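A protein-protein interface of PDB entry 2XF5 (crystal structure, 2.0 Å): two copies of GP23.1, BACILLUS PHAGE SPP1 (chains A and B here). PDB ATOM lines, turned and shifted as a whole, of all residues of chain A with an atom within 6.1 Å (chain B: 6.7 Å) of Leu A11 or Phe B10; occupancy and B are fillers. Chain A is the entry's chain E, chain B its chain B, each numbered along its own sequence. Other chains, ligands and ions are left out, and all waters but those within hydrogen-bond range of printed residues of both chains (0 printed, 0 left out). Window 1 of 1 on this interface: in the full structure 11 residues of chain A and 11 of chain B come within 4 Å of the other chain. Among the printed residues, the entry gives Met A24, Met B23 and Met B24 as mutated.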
ATOM      1  N   LEU A   6     -32.106 -37.599 -24.575  1.00  0.00           N
ATOM      2  CA  LEU A   6     -31.068 -36.778 -25.202  1.00  0.00           C
ATOM      3  C   LEU A   6     -31.324 -35.287 -25.188  1.00  0.00           C
ATOM      4  O   LEU A   6     -30.608 -34.542 -25.867  1.00  0.00           O
ATOM      5  CB  LEU A   6     -30.743 -37.291 -26.609  1.00  0.00           C
ATOM      6  CG  LEU A   6     -30.256 -38.729 -26.697  1.00  0.00           C
ATOM      7  CD1 LEU A   6     -30.237 -39.197 -28.142  1.00  0.00           C
ATOM      8  CD2 LEU A   6     -28.892 -38.886 -26.091  1.00  0.00           C
ATOM      9  N   TYR A   7     -32.281 -34.826 -24.339  1.00  0.00           N
ATOM     10  CA  TYR A   7     -32.583 -33.402 -24.232  1.00  0.00           C
ATOM     11  C   TYR A   7     -31.314 -32.600 -23.869  1.00  0.00           C
ATOM     12  O   TYR A   7     -30.943 -31.679 -24.597  1.00  0.00           O
ATOM     13  CB  TYR A   7     -33.718 -33.125 -23.226  1.00  0.00           C
ATOM     14  CG  TYR A   7     -34.028 -31.647 -23.147  1.00  0.00           C
ATOM     15  CD1 TYR A   7     -34.761 -31.013 -24.148  1.00  0.00           C
ATOM     16  CD2 TYR A   7     -33.511 -30.858 -22.120  1.00  0.00           C
ATOM     17  CE1 TYR A   7     -35.025 -29.645 -24.101  1.00  0.00           C
ATOM     18  CE2 TYR A   7     -33.725 -29.483 -22.090  1.00  0.00           C
ATOM     19  CZ  TYR A   7     -34.471 -28.877 -23.100  1.00  0.00           C
ATOM     20  OH  TYR A   7     -34.739 -27.527 -23.086  1.00  0.00           O
ATOM     21  N   GLY A   8     -30.668 -32.973 -22.774  1.00  0.00           N
ATOM     22  CA  GLY A   8     -29.449 -32.323 -22.296  1.00  0.00           C
ATOM     23  C   GLY A   8     -28.334 -32.367 -23.314  1.00  0.00           C
ATOM     24  O   GLY A   8     -27.634 -31.379 -23.510  1.00  0.00           O
ATOM     25  N   TYR A   9     -28.182 -33.515 -23.997  1.00  0.00           N
ATOM     26  CA  TYR A   9     -27.172 -33.733 -25.025  1.00  0.00           C
ATOM     27  C   TYR A   9     -27.355 -32.730 -26.184  1.00  0.00           C
ATOM     28  O   TYR A   9     -26.372 -32.096 -26.603  1.00  0.00           O
ATOM     29  CB  TYR A   9     -27.256 -35.177 -25.557  1.00  0.00           C
ATOM     30  CG  TYR A   9     -26.299 -35.453 -26.695  1.00  0.00           C
ATOM     31  CD1 TYR A   9     -24.945 -35.695 -26.454  1.00  0.00           C
ATOM     32  CD2 TYR A   9     -26.747 -35.498 -28.013  1.00  0.00           C
ATOM     33  CE1 TYR A   9     -24.050 -35.903 -27.499  1.00  0.00           C
ATOM     34  CE2 TYR A   9     -25.866 -35.757 -29.067  1.00  0.00           C
ATOM     35  CZ  TYR A   9     -24.518 -35.954 -28.806  1.00  0.00           C
ATOM     36  OH  TYR A   9     -23.650 -36.204 -29.844  1.00  0.00           O
ATOM     37  N   PHE A  10     -28.598 -32.595 -26.698  1.00  0.00           N
ATOM     38  CA  PHE A  10     -28.865 -31.663 -27.791  1.00  0.00           C
ATOM     39  C   PHE A  10     -28.844 -30.213 -27.337  1.00  0.00           C
ATOM     40  O   PHE A  10     -28.379 -29.360 -28.096  1.00  0.00           O
ATOM     41  CB  PHE A  10     -30.146 -32.023 -28.573  1.00  0.00           C
ATOM     42  CG  PHE A  10     -29.998 -33.259 -29.424  1.00  0.00           C
ATOM     43  CD1 PHE A  10     -29.160 -33.266 -30.538  1.00  0.00           C
ATOM     44  CD2 PHE A  10     -30.720 -34.416 -29.136  1.00  0.00           C
ATOM     45  CE1 PHE A  10     -29.022 -34.417 -31.317  1.00  0.00           C
ATOM     46  CE2 PHE A  10     -30.575 -35.560 -29.922  1.00  0.00           C
ATOM     47  CZ  PHE A  10     -29.743 -35.548 -31.008  1.00  0.00           C
ATOM     48  N   LEU A  11     -29.292 -29.921 -26.086  1.00  0.00           N
ATOM     49  CA  LEU A  11     -29.246 -28.551 -25.577  1.00  0.00           C
ATOM     50  C   LEU A  11     -27.785 -28.099 -25.494  1.00  0.00           C
ATOM     51  O   LEU A  11     -27.457 -27.001 -25.930  1.00  0.00           O
ATOM     52  CB  LEU A  11     -29.930 -28.423 -24.208  1.00  0.00           C
ATOM     53  CG  LEU A  11     -29.794 -27.045 -23.514  1.00  0.00           C
ATOM     54  CD1 LEU A  11     -30.448 -25.946 -24.346  1.00  0.00           C
ATOM     55  CD2 LEU A  11     -30.371 -27.076 -22.143  1.00  0.00           C
ATOM     56  N   ASP A  12     -26.919 -28.957 -24.973  1.00  0.00           N
ATOM     57  CA  ASP A  12     -25.486 -28.670 -24.859  1.00  0.00           C
ATOM     58  C   ASP A  12     -24.860 -28.444 -26.253  1.00  0.00           C
ATOM     59  O   ASP A  12     -24.048 -27.540 -26.397  1.00  0.00           O
ATOM     60  CB  ASP A  12     -24.761 -29.800 -24.124  1.00  0.00           C
ATOM     61  CG  ASP A  12     -23.269 -29.543 -23.970  1.00  0.00           C
ATOM     62  OD1 ASP A  12     -22.911 -28.621 -23.242  1.00  0.00           O
ATOM     63  OD2 ASP A  12     -22.472 -30.216 -24.664  1.00  0.00           O
ATOM     64  N   SER A  13     -25.278 -29.222 -27.276  1.00  0.00           N
ATOM     65  CA  SER A  13     -24.726 -29.065 -28.631  1.00  0.00           C
ATOM     66  C   SER A  13     -25.171 -27.738 -29.266  1.00  0.00           C
ATOM     67  O   SER A  13     -24.425 -27.138 -30.044  1.00  0.00           O
ATOM     68  CB  SER A  13     -25.061 -30.263 -29.516  1.00  0.00           C
ATOM     69  OG  SER A  13     -26.440 -30.298 -29.849  1.00  0.00           O
ATOM     70  N   TRP A  14     -26.381 -27.274 -28.922  1.00  0.00           N
ATOM     71  CA  TRP A  14     -26.916 -25.996 -29.401  1.00  0.00           C
ATOM     72  C   TRP A  14     -26.153 -24.863 -28.715  1.00  0.00           C
ATOM     73  O   TRP A  14     -25.696 -23.945 -29.391  1.00  0.00           O
ATOM     74  CB  TRP A  14     -28.410 -25.907 -29.098  1.00  0.00           C
ATOM     75  CG  TRP A  14     -29.057 -24.625 -29.539  1.00  0.00           C
ATOM     76  CD1 TRP A  14     -29.258 -23.507 -28.785  1.00  0.00           C
ATOM     77  CD2 TRP A  14     -29.564 -24.323 -30.849  1.00  0.00           C
ATOM     78  NE1 TRP A  14     -29.846 -22.521 -29.546  1.00  0.00           N
ATOM     79  CE2 TRP A  14     -30.054 -23.000 -30.815  1.00  0.00           C
ATOM     80  CE3 TRP A  14     -29.673 -25.054 -32.042  1.00  0.00           C
ATOM     81  CZ2 TRP A  14     -30.636 -22.387 -31.933  1.00  0.00           C
ATOM     82  CZ3 TRP A  14     -30.224 -24.437 -33.158  1.00  0.00           C
ATOM     83  CH2 TRP A  14     -30.697 -23.120 -33.097  1.00  0.00           C
ATOM     84  N   LEU A  15     -25.967 -24.955 -27.376  1.00  0.00           N
ATOM     85  CA  LEU A  15     -25.239 -23.957 -26.590  1.00  0.00           C
ATOM     86  C   LEU A  15     -23.755 -23.918 -26.930  1.00  0.00           C
ATOM     87  O   LEU A  15     -23.136 -22.870 -26.841  1.00  0.00           O
ATOM     88  CB  LEU A  15     -25.450 -24.170 -25.084  1.00  0.00           C
ATOM     89  CG  LEU A  15     -26.860 -23.880 -24.564  1.00  0.00           C
ATOM     90  CD1 LEU A  15     -27.032 -24.386 -23.160  1.00  0.00           C
ATOM     91  CD2 LEU A  15     -27.184 -22.429 -24.647  1.00  0.00           C
ATOM     92  N   ASP A  16     -23.198 -25.047 -27.332  1.00  0.00           N
ATOM     93  CA  ASP A  16     -21.795 -25.150 -27.736  1.00  0.00           C
ATOM     94  C   ASP A  16     -21.555 -24.608 -29.160  1.00  0.00           C
ATOM     95  O   ASP A  16     -20.403 -24.395 -29.527  1.00  0.00           O
ATOM     96  CB  ASP A  16     -21.336 -26.622 -27.679  1.00  0.00           C
ATOM     97  CG  ASP A  16     -20.093 -26.893 -26.850  1.00  0.00           C
ATOM     98  OD1 ASP A  16     -19.264 -25.964 -26.697  1.00  0.00           O
ATOM     99  OD2 ASP A  16     -19.926 -28.048 -26.387  1.00  0.00           O
ATOM    100  N   MET A  24     -31.545 -30.177 -35.232  1.00  0.00           N
ATOM    101  CA  MET A  24     -32.652 -30.216 -34.282  1.00  0.00           C
ATOM    102  C   MET A  24     -33.881 -30.867 -34.927  1.00  0.00           C
ATOM    103  O   MET A  24     -34.531 -31.698 -34.299  1.00  0.00           O
ATOM    104  CB  MET A  24     -32.978 -28.807 -33.755  1.00  0.00           C
ATOM    105  CG  MET A  24     -31.821 -28.131 -33.014  1.00  0.00           C
ATOM    106  SD  MET A  24     -31.225 -29.131 -31.427  1.00  0.00           S
ATOM    107  CE  MET A  24     -29.895 -30.220 -32.198  1.00  0.00           C
ATOM    108  N   LYS A  40     -37.964 -25.482 -27.480  1.00  0.00           N
ATOM    109  CA  LYS A  40     -37.399 -25.034 -26.188  1.00  0.00           C
ATOM    110  C   LYS A  40     -35.894 -24.812 -26.356  1.00  0.00           C
ATOM    111  O   LYS A  40     -35.404 -23.768 -25.966  1.00  0.00           O
ATOM    112  CB  LYS A  40     -37.613 -26.105 -25.100  1.00  0.00           C
ATOM    113  CG  LYS A  40     -38.464 -25.688 -23.922  1.00  0.00           C
ATOM    114  CD  LYS A  40     -38.947 -26.881 -23.057  1.00  0.00           C
ATOM    115  CE  LYS A  40     -37.844 -27.738 -22.467  1.00  0.00           C
ATOM    116  NZ  LYS A  40     -38.278 -28.468 -21.248  1.00  0.00           N
ATOM    117  N   ILE A  41     -35.171 -25.774 -26.955  1.00  0.00           N
ATOM    118  CA  ILE A  41     -33.709 -25.692 -27.151  1.00  0.00           C
ATOM    119  C   ILE A  41     -33.349 -24.478 -28.013  1.00  0.00           C
ATOM    120  O   ILE A  41     -32.462 -23.707 -27.649  1.00  0.00           O
ATOM    121  CB  ILE A  41     -33.105 -27.013 -27.688  1.00  0.00           C
ATOM    122  CG1 ILE A  41     -33.131 -28.119 -26.613  1.00  0.00           C
ATOM    123  CG2 ILE A  41     -31.670 -26.799 -28.186  1.00  0.00           C
ATOM    124  CD1 ILE A  41     -32.869 -29.564 -27.122  1.00  0.00           C
ATOM    125  N   TYR A  44     -32.930 -20.868 -26.700  1.00  0.00           N
ATOM    126  CA  TYR A  44     -31.660 -20.502 -26.062  1.00  0.00           C
ATOM    127  C   TYR A  44     -30.748 -19.841 -27.092  1.00  0.00           C
ATOM    128  O   TYR A  44     -30.845 -20.184 -28.279  1.00  0.00           O
ATOM    129  CB  TYR A  44     -30.933 -21.744 -25.538  1.00  0.00           C
ATOM    130  CG  TYR A  44     -31.466 -22.309 -24.245  1.00  0.00           C
ATOM    131  CD1 TYR A  44     -30.808 -22.083 -23.036  1.00  0.00           C
ATOM    132  CD2 TYR A  44     -32.578 -23.142 -24.236  1.00  0.00           C
ATOM    133  CE1 TYR A  44     -31.265 -22.651 -21.849  1.00  0.00           C
ATOM    134  CE2 TYR A  44     -33.033 -23.724 -23.058  1.00  0.00           C
ATOM    135  CZ  TYR A  44     -32.362 -23.494 -21.873  1.00  0.00           C
ATOM    136  OH  TYR A  44     -32.818 -24.115 -20.743  1.00  0.00           O
ATOM    137  N   TRP A  49     -22.050 -20.764 -25.268  1.00  0.00           N
ATOM    138  CA  TRP A  49     -20.930 -21.221 -24.494  1.00  0.00           C
ATOM    139  C   TRP A  49     -19.668 -20.724 -25.111  1.00  0.00           C
ATOM    140  O   TRP A  49     -18.599 -21.134 -24.733  1.00  0.00           O
ATOM    141  CB  TRP A  49     -20.882 -22.721 -24.387  1.00  0.00           C
ATOM    142  CG  TRP A  49     -21.855 -23.333 -23.464  1.00  0.00           C
ATOM    143  CD1 TRP A  49     -22.051 -24.633 -23.278  1.00  0.00           C
ATOM    144  CD2 TRP A  49     -22.742 -22.660 -22.570  1.00  0.00           C
ATOM    145  NE1 TRP A  49     -23.019 -24.839 -22.369  1.00  0.00           N
ATOM    146  CE2 TRP A  49     -23.466 -23.637 -21.908  1.00  0.00           C
ATOM    147  CE3 TRP A  49     -23.000 -21.329 -22.282  1.00  0.00           C
ATOM    148  CZ2 TRP A  49     -24.412 -23.333 -20.949  1.00  0.00           C
ATOM    149  CZ3 TRP A  49     -23.949 -21.028 -21.350  1.00  0.00           C
ATOM    150  CH2 TRP A  49     -24.644 -22.021 -20.692  1.00  0.00           C
ATOM    151  N   LEU B   6     -31.028 -30.528 -15.178  1.00  0.00           N
ATOM    152  CA  LEU B   6     -29.934 -29.661 -15.621  1.00  0.00           C
ATOM    153  C   LEU B   6     -29.380 -28.716 -14.582  1.00  0.00           C
ATOM    154  O   LEU B   6     -28.597 -27.833 -14.930  1.00  0.00           O
ATOM    155  CB  LEU B   6     -30.310 -28.939 -16.920  1.00  0.00           C
ATOM    156  CG  LEU B   6     -30.665 -29.855 -18.101  1.00  0.00           C
ATOM    157  CD1 LEU B   6     -31.297 -29.073 -19.209  1.00  0.00           C
ATOM    158  CD2 LEU B   6     -29.442 -30.649 -18.600  1.00  0.00           C
ATOM    159  N   TYR B   7     -29.739 -28.919 -13.293  1.00  0.00           N
ATOM    160  CA  TYR B   7     -29.242 -28.058 -12.220  1.00  0.00           C
ATOM    161  C   TYR B   7     -27.686 -27.986 -12.212  1.00  0.00           C
ATOM    162  O   TYR B   7     -27.118 -26.889 -12.293  1.00  0.00           O
ATOM    163  CB  TYR B   7     -29.774 -28.497 -10.840  1.00  0.00           C
ATOM    164  CG  TYR B   7     -29.249 -27.579  -9.757  1.00  0.00           C
ATOM    165  CD1 TYR B   7     -29.809 -26.330  -9.551  1.00  0.00           C
ATOM    166  CD2 TYR B   7     -28.120 -27.924  -9.002  1.00  0.00           C
ATOM    167  CE1 TYR B   7     -29.302 -25.460  -8.591  1.00  0.00           C
ATOM    168  CE2 TYR B   7     -27.591 -27.046  -8.050  1.00  0.00           C
ATOM    169  CZ  TYR B   7     -28.173 -25.803  -7.868  1.00  0.00           C
ATOM    170  OH  TYR B   7     -27.681 -24.927  -6.918  1.00  0.00           O
ATOM    171  N   GLY B   8     -27.030 -29.151 -12.169  1.00  0.00           N
ATOM    172  CA  GLY B   8     -25.570 -29.250 -12.159  1.00  0.00           C
ATOM    173  C   GLY B   8     -24.945 -28.641 -13.395  1.00  0.00           C
ATOM    174  O   GLY B   8     -23.922 -27.950 -13.322  1.00  0.00           O
ATOM    175  N   TYR B   9     -25.602 -28.857 -14.534  1.00  0.00           N
ATOM    176  CA  TYR B   9     -25.162 -28.363 -15.834  1.00  0.00           C
ATOM    177  C   TYR B   9     -25.127 -26.837 -15.851  1.00  0.00           C
ATOM    178  O   TYR B   9     -24.125 -26.243 -16.262  1.00  0.00           O
ATOM    179  CB  TYR B   9     -26.075 -28.931 -16.944  1.00  0.00           C
ATOM    180  CG  TYR B   9     -25.709 -28.422 -18.307  1.00  0.00           C
ATOM    181  CD1 TYR B   9     -24.633 -28.968 -19.012  1.00  0.00           C
ATOM    182  CD2 TYR B   9     -26.437 -27.391 -18.908  1.00  0.00           C
ATOM    183  CE1 TYR B   9     -24.296 -28.509 -20.285  1.00  0.00           C
ATOM    184  CE2 TYR B   9     -26.094 -26.908 -20.169  1.00  0.00           C
ATOM    185  CZ  TYR B   9     -25.034 -27.483 -20.860  1.00  0.00           C
ATOM    186  OH  TYR B   9     -24.665 -26.998 -22.092  1.00  0.00           O
ATOM    187  N   PHE B  10     -26.213 -26.203 -15.394  1.00  0.00           N
ATOM    188  CA  PHE B  10     -26.294 -24.740 -15.329  1.00  0.00           C
ATOM    189  C   PHE B  10     -25.431 -24.141 -14.229  1.00  0.00           C
ATOM    190  O   PHE B  10     -24.848 -23.070 -14.442  1.00  0.00           O
ATOM    191  CB  PHE B  10     -27.736 -24.222 -15.311  1.00  0.00           C
ATOM    192  CG  PHE B  10     -28.432 -24.389 -16.647  1.00  0.00           C
ATOM    193  CD1 PHE B  10     -28.011 -23.678 -17.768  1.00  0.00           C
ATOM    194  CD2 PHE B  10     -29.509 -25.249 -16.781  1.00  0.00           C
ATOM    195  CE1 PHE B  10     -28.656 -23.838 -19.004  1.00  0.00           C
ATOM    196  CE2 PHE B  10     -30.166 -25.388 -18.004  1.00  0.00           C
ATOM    197  CZ  PHE B  10     -29.725 -24.695 -19.112  1.00  0.00           C
ATOM    198  N   LEU B  11     -25.286 -24.852 -13.073  1.00  0.00           N
ATOM    199  CA  LEU B  11     -24.417 -24.363 -12.001  1.00  0.00           C
ATOM    200  C   LEU B  11     -22.966 -24.293 -12.519  1.00  0.00           C
ATOM    201  O   LEU B  11     -22.272 -23.298 -12.308  1.00  0.00           O
ATOM    202  CB  LEU B  11     -24.483 -25.286 -10.755  1.00  0.00           C
ATOM    203  CG  LEU B  11     -23.482 -24.966  -9.633  1.00  0.00           C
ATOM    204  CD1 LEU B  11     -23.681 -23.540  -9.117  1.00  0.00           C
ATOM    205  CD2 LEU B  11     -23.589 -25.954  -8.527  1.00  0.00           C
ATOM    206  N   ASP B  12     -22.547 -25.329 -13.241  1.00  0.00           N
ATOM    207  CA  ASP B  12     -21.199 -25.401 -13.810  1.00  0.00           C
ATOM    208  C   ASP B  12     -20.991 -24.239 -14.808  1.00  0.00           C
ATOM    209  O   ASP B  12     -19.921 -23.645 -14.816  1.00  0.00           O
ATOM    210  CB  ASP B  12     -20.968 -26.773 -14.470  1.00  0.00           C
ATOM    211  CG  ASP B  12     -19.571 -26.920 -15.032  1.00  0.00           C
ATOM    212  OD1 ASP B  12     -18.603 -26.894 -14.230  1.00  0.00           O
ATOM    213  OD2 ASP B  12     -19.436 -26.976 -16.270  1.00  0.00           O
ATOM    214  N   SER B  13     -22.003 -23.924 -15.630  1.00  0.00           N
ATOM    215  CA  SER B  13     -21.887 -22.835 -16.619  1.00  0.00           C
ATOM    216  C   SER B  13     -21.780 -21.454 -15.951  1.00  0.00           C
ATOM    217  O   SER B  13     -21.112 -20.553 -16.477  1.00  0.00           O
ATOM    218  CB  SER B  13     -23.030 -22.872 -17.630  1.00  0.00           C
ATOM    219  OG  SER B  13     -24.260 -22.503 -17.030  1.00  0.00           O
ATOM    220  N   TRP B  14     -22.436 -21.285 -14.784  1.00  0.00           N
ATOM    221  CA  TRP B  14     -22.374 -20.055 -14.025  1.00  0.00           C
ATOM    222  C   TRP B  14     -20.965 -19.897 -13.421  1.00  0.00           C
ATOM    223  O   TRP B  14     -20.369 -18.823 -13.532  1.00  0.00           O
ATOM    224  CB  TRP B  14     -23.447 -20.054 -12.929  1.00  0.00           C
ATOM    225  CG  TRP B  14     -23.445 -18.822 -12.068  1.00  0.00           C
ATOM    226  CD1 TRP B  14     -22.824 -18.672 -10.860  1.00  0.00           C
ATOM    227  CD2 TRP B  14     -24.128 -17.585 -12.328  1.00  0.00           C
ATOM    228  NE1 TRP B  14     -23.056 -17.405 -10.365  1.00  0.00           N
ATOM    229  CE2 TRP B  14     -23.852 -16.718 -11.246  1.00  0.00           C
ATOM    230  CE3 TRP B  14     -24.964 -17.124 -13.369  1.00  0.00           C
ATOM    231  CZ2 TRP B  14     -24.364 -15.416 -11.182  1.00  0.00           C
ATOM    232  CZ3 TRP B  14     -25.482 -15.836 -13.297  1.00  0.00           C
ATOM    233  CH2 TRP B  14     -25.159 -14.989 -12.230  1.00  0.00           C
ATOM    234  N   LEU B  15     -20.433 -20.977 -12.814  1.00  0.00           N
ATOM    235  CA  LEU B  15     -19.098 -21.015 -12.213  1.00  0.00           C
ATOM    236  C   LEU B  15     -18.017 -20.819 -13.273  1.00  0.00           C
ATOM    237  O   LEU B  15     -16.979 -20.228 -12.984  1.00  0.00           O
ATOM    238  CB  LEU B  15     -18.879 -22.330 -11.442  1.00  0.00           C
ATOM    239  CG  LEU B  15     -19.681 -22.467 -10.135  1.00  0.00           C
ATOM    240  CD1 LEU B  15     -19.578 -23.893  -9.591  1.00  0.00           C
ATOM    241  CD2 LEU B  15     -19.263 -21.410  -9.069  1.00  0.00           C
ATOM    242  N   ALA B  19     -22.475 -18.636 -18.415  1.00  0.00           N
ATOM    243  CA  ALA B  19     -23.851 -18.233 -18.182  1.00  0.00           C
ATOM    244  C   ALA B  19     -23.934 -16.896 -17.424  1.00  0.00           C
ATOM    245  O   ALA B  19     -23.095 -16.648 -16.589  1.00  0.00           O
ATOM    246  CB  ALA B  19     -24.576 -19.330 -17.383  1.00  0.00           C
ATOM    247  N   MET B  23     -29.068 -16.273 -19.338  1.00  0.00           N
ATOM    248  CA  MET B  23     -29.229 -17.709 -19.528  1.00  0.00           C
ATOM    249  C   MET B  23     -30.151 -18.289 -18.456  1.00  0.00           C
ATOM    250  O   MET B  23     -30.968 -19.155 -18.754  1.00  0.00           O
ATOM    251  CB  MET B  23     -27.848 -18.360 -19.419  1.00  0.00           C
ATOM    252  CG  MET B  23     -27.846 -19.857 -19.629  1.00  0.00           C
ATOM    253  SD  MET B  23     -28.473 -20.257 -21.403  1.00  0.00           S
ATOM    254  CE  MET B  23     -27.166 -19.258 -22.402  1.00  0.00           C
ATOM    255  N   MET B  24     -29.988 -17.830 -17.204  1.00  0.00           N
ATOM    256  CA  MET B  24     -30.772 -18.263 -16.038  1.00  0.00           C
ATOM    257  C   MET B  24     -32.281 -18.002 -16.354  1.00  0.00           C
ATOM    258  O   MET B  24     -33.097 -18.901 -16.159  1.00  0.00           O
ATOM    259  CB  MET B  24     -30.271 -17.551 -14.753  1.00  0.00           C
ATOM    260  CG  MET B  24     -28.810 -17.895 -14.382  1.00  0.00           C
ATOM    261  SD  MET B  24     -28.617 -19.814 -13.964  1.00  0.00           S
ATOM    262  CE  MET B  24     -28.092 -20.442 -15.717  1.00  0.00           C
ATOM    263  N   ALA B  27     -33.549 -20.519 -19.159  1.00  0.00           N
ATOM    264  CA  ALA B  27     -33.736 -21.845 -18.562  1.00  0.00           C
ATOM    265  C   ALA B  27     -34.998 -21.906 -17.681  1.00  0.00           C
ATOM    266  O   ALA B  27     -35.769 -22.856 -17.811  1.00  0.00           O
ATOM    267  CB  ALA B  27     -32.491 -22.248 -17.766  1.00  0.00           C
ATOM    268  N   ASP B  32     -36.417 -25.644 -17.590  1.00  0.00           N
ATOM    269  CA  ASP B  32     -35.206 -26.435 -17.351  1.00  0.00           C
ATOM    270  C   ASP B  32     -34.593 -26.148 -15.971  1.00  0.00           C
ATOM    271  O   ASP B  32     -33.778 -26.924 -15.466  1.00  0.00           O
ATOM    272  CB  ASP B  32     -34.194 -26.227 -18.483  1.00  0.00           C
ATOM    273  CG  ASP B  32     -34.707 -26.785 -19.812  1.00  0.00           C
ATOM    274  OD1 ASP B  32     -35.492 -27.764 -19.784  1.00  0.00           O
ATOM    275  OD2 ASP B  32     -34.361 -26.209 -20.868  1.00  0.00           O
ATOM    276  N   LEU B  33     -35.062 -25.066 -15.340  1.00  0.00           N
ATOM    277  CA  LEU B  33     -34.660 -24.671 -14.000  1.00  0.00           C
ATOM    278  C   LEU B  33     -35.886 -24.047 -13.329  1.00  0.00           C
ATOM    279  O   LEU B  33     -36.708 -23.428 -14.032  1.00  0.00           O
ATOM    280  CB  LEU B  33     -33.567 -23.573 -14.083  1.00  0.00           C
ATOM    281  CG  LEU B  33     -32.102 -23.946 -14.346  1.00  0.00           C
ATOM    282  CD1 LEU B  33     -31.199 -22.722 -14.046  1.00  0.00           C
ATOM    283  CD2 LEU B  33     -31.646 -25.115 -13.480  1.00  0.00           C
ATOM    284  N   ILE B  41     -28.186 -20.941  -7.820  1.00  0.00           N
ATOM    285  CA  ILE B  41     -27.026 -20.877  -8.724  1.00  0.00           C
ATOM    286  C   ILE B  41     -26.394 -19.486  -8.661  1.00  0.00           C
ATOM    287  O   ILE B  41     -25.186 -19.374  -8.500  1.00  0.00           O
ATOM    288  CB  ILE B  41     -27.387 -21.320 -10.175  1.00  0.00           C
ATOM    289  CG1 ILE B  41     -27.659 -22.848 -10.234  1.00  0.00           C
ATOM    290  CG2 ILE B  41     -26.275 -20.955 -11.142  1.00  0.00           C
ATOM    291  CD1 ILE B  41     -28.339 -23.387 -11.502  1.00  0.00           C
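The side-chain hydroxyl (OH) of Tyr B9 is in hydrogen-bond range of the indole nitrogen (NE1) of Trp A49 (2.7 Å). OD1 of Asp A12 lies within hydrogen-bond range of OH of Tyr B9 (2.7 Å). NZ of Lys A40 is in salt-bridge range of OD1 of Asp B32 (3.2 Å). OD2 of Asp B32 is in hydrogen-bond range of OH of Tyr A44. The side-chain hydroxyl (OH) of Tyr A7 sits at hydrogen-bond distance from the side-chain carboxylate (OD2) of Asp B32 (2.6 Å).
Tyr A7 touches Leu B6, but with the chains exchanged Leu A6 does not touch Tyr B7 (13.6 Å). Leu A11 touches Leu B6, but with the chains exchanged Leu A6 does not touch Leu B11 (16.9 Å). Asp A12 touches Tyr B9, but with the chains exchanged Tyr A9 does not touch Asp B12 (13.4 Å). Leu A15 touches Tyr B9, but with the chains exchanged Tyr A9 does not touch Leu B15 (18.5 Å). 12 positions are printed for both chains. Of the 15 pairs that touch across the chains among the printed residues, none has its exchanged pair printed and touching as well.
Of chain B, only Leu B6 (3.7 Å) and Phe B10 (3.9 Å) come within 4 Å of Leu A11. Phe B10 touches two residues of chain A. Of the printed residues of chain B, Tyr A44 touches Phe B10 (3.5 Å), Met B23 (3.4 Å), Ala B27 (3.3 Å) and Asp B32 (2.6 Å). Of the printed residues of chain A, Ala B27 touches Tyr A44 (3.3 Å). Leu B33 touches none of the printed residues of chain A. Asp B12 touches none of the printed residues of chain A. The nearest residue of chain A that does not touch Phe B10 is Leu A15 (4.5 Å). The nearest printed residue of chain A that does not touch Met B23 is Leu A11 (6.7 Å).
The backbone carbonyl oxygen (O) of Phe B10 is in hydrogen-bond range of the side-chain hydroxyl (OG) of Ser B13, at 2.7 Å. The backbone carbonyl oxygen (O) of Leu A15 sits at hydrogen-bond distance from the backbone NH (N) of Trp A49 (2.8 Å). O of Ala B27 sits at hydrogen-bond distance from N of Asp B32 (2.9 Å). The backbone carbonyl oxygen (O) of Ser B13 sits at hydrogen-bond distance from the backbone NH (N) of Ala B19 (3.0 Å). The backbone carbonyl oxygen (O) of Tyr A44 is in hydrogen-bond range of the indole nitrogen (NE1) of Trp A14 (2.8 Å). O of Ala B27 sits at hydrogen-bond distance from N of Leu B33 (3.4 Å).
Printed residues of chain B that touch a printed residue of chain A: Leu B6, Tyr B9, Phe B10, Ser B13, Met B23, Ala B27 and Asp B32. Along chain B the printed residues that touch a printed residue of chain A span positions 6 to 32. Of the 16 printed residues of chain A, 7 touch a printed residue of chain B. Hydrophobic or aromatic side chains of chain A that line the printed part of chain B: Tyr A7, Leu A11, Leu A15, Tyr A44 and Trp A49. Along chain A the printed residues that touch a printed residue of chain B span positions 7 to 49. Among the printed residues, Asp or Glu carboxylates within 4 Å of a Lys or Arg side-chain nitrogen of the other chain: Lys A40 with Asp B32 (3.2 Å).
Among the printed residues, pairs that only touch across the chains: Tyr A7 with Leu B6, Leu A11 with Leu B6, Leu A11 with Phe B10, Leu A15 with Tyr B9, Leu A15 with Met B23, Tyr A44 with Phe B10, Tyr A44 with Met B23, Tyr A44 with Ala B27, Trp A49 with Ser B13 and Trp A49 with Met B23.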
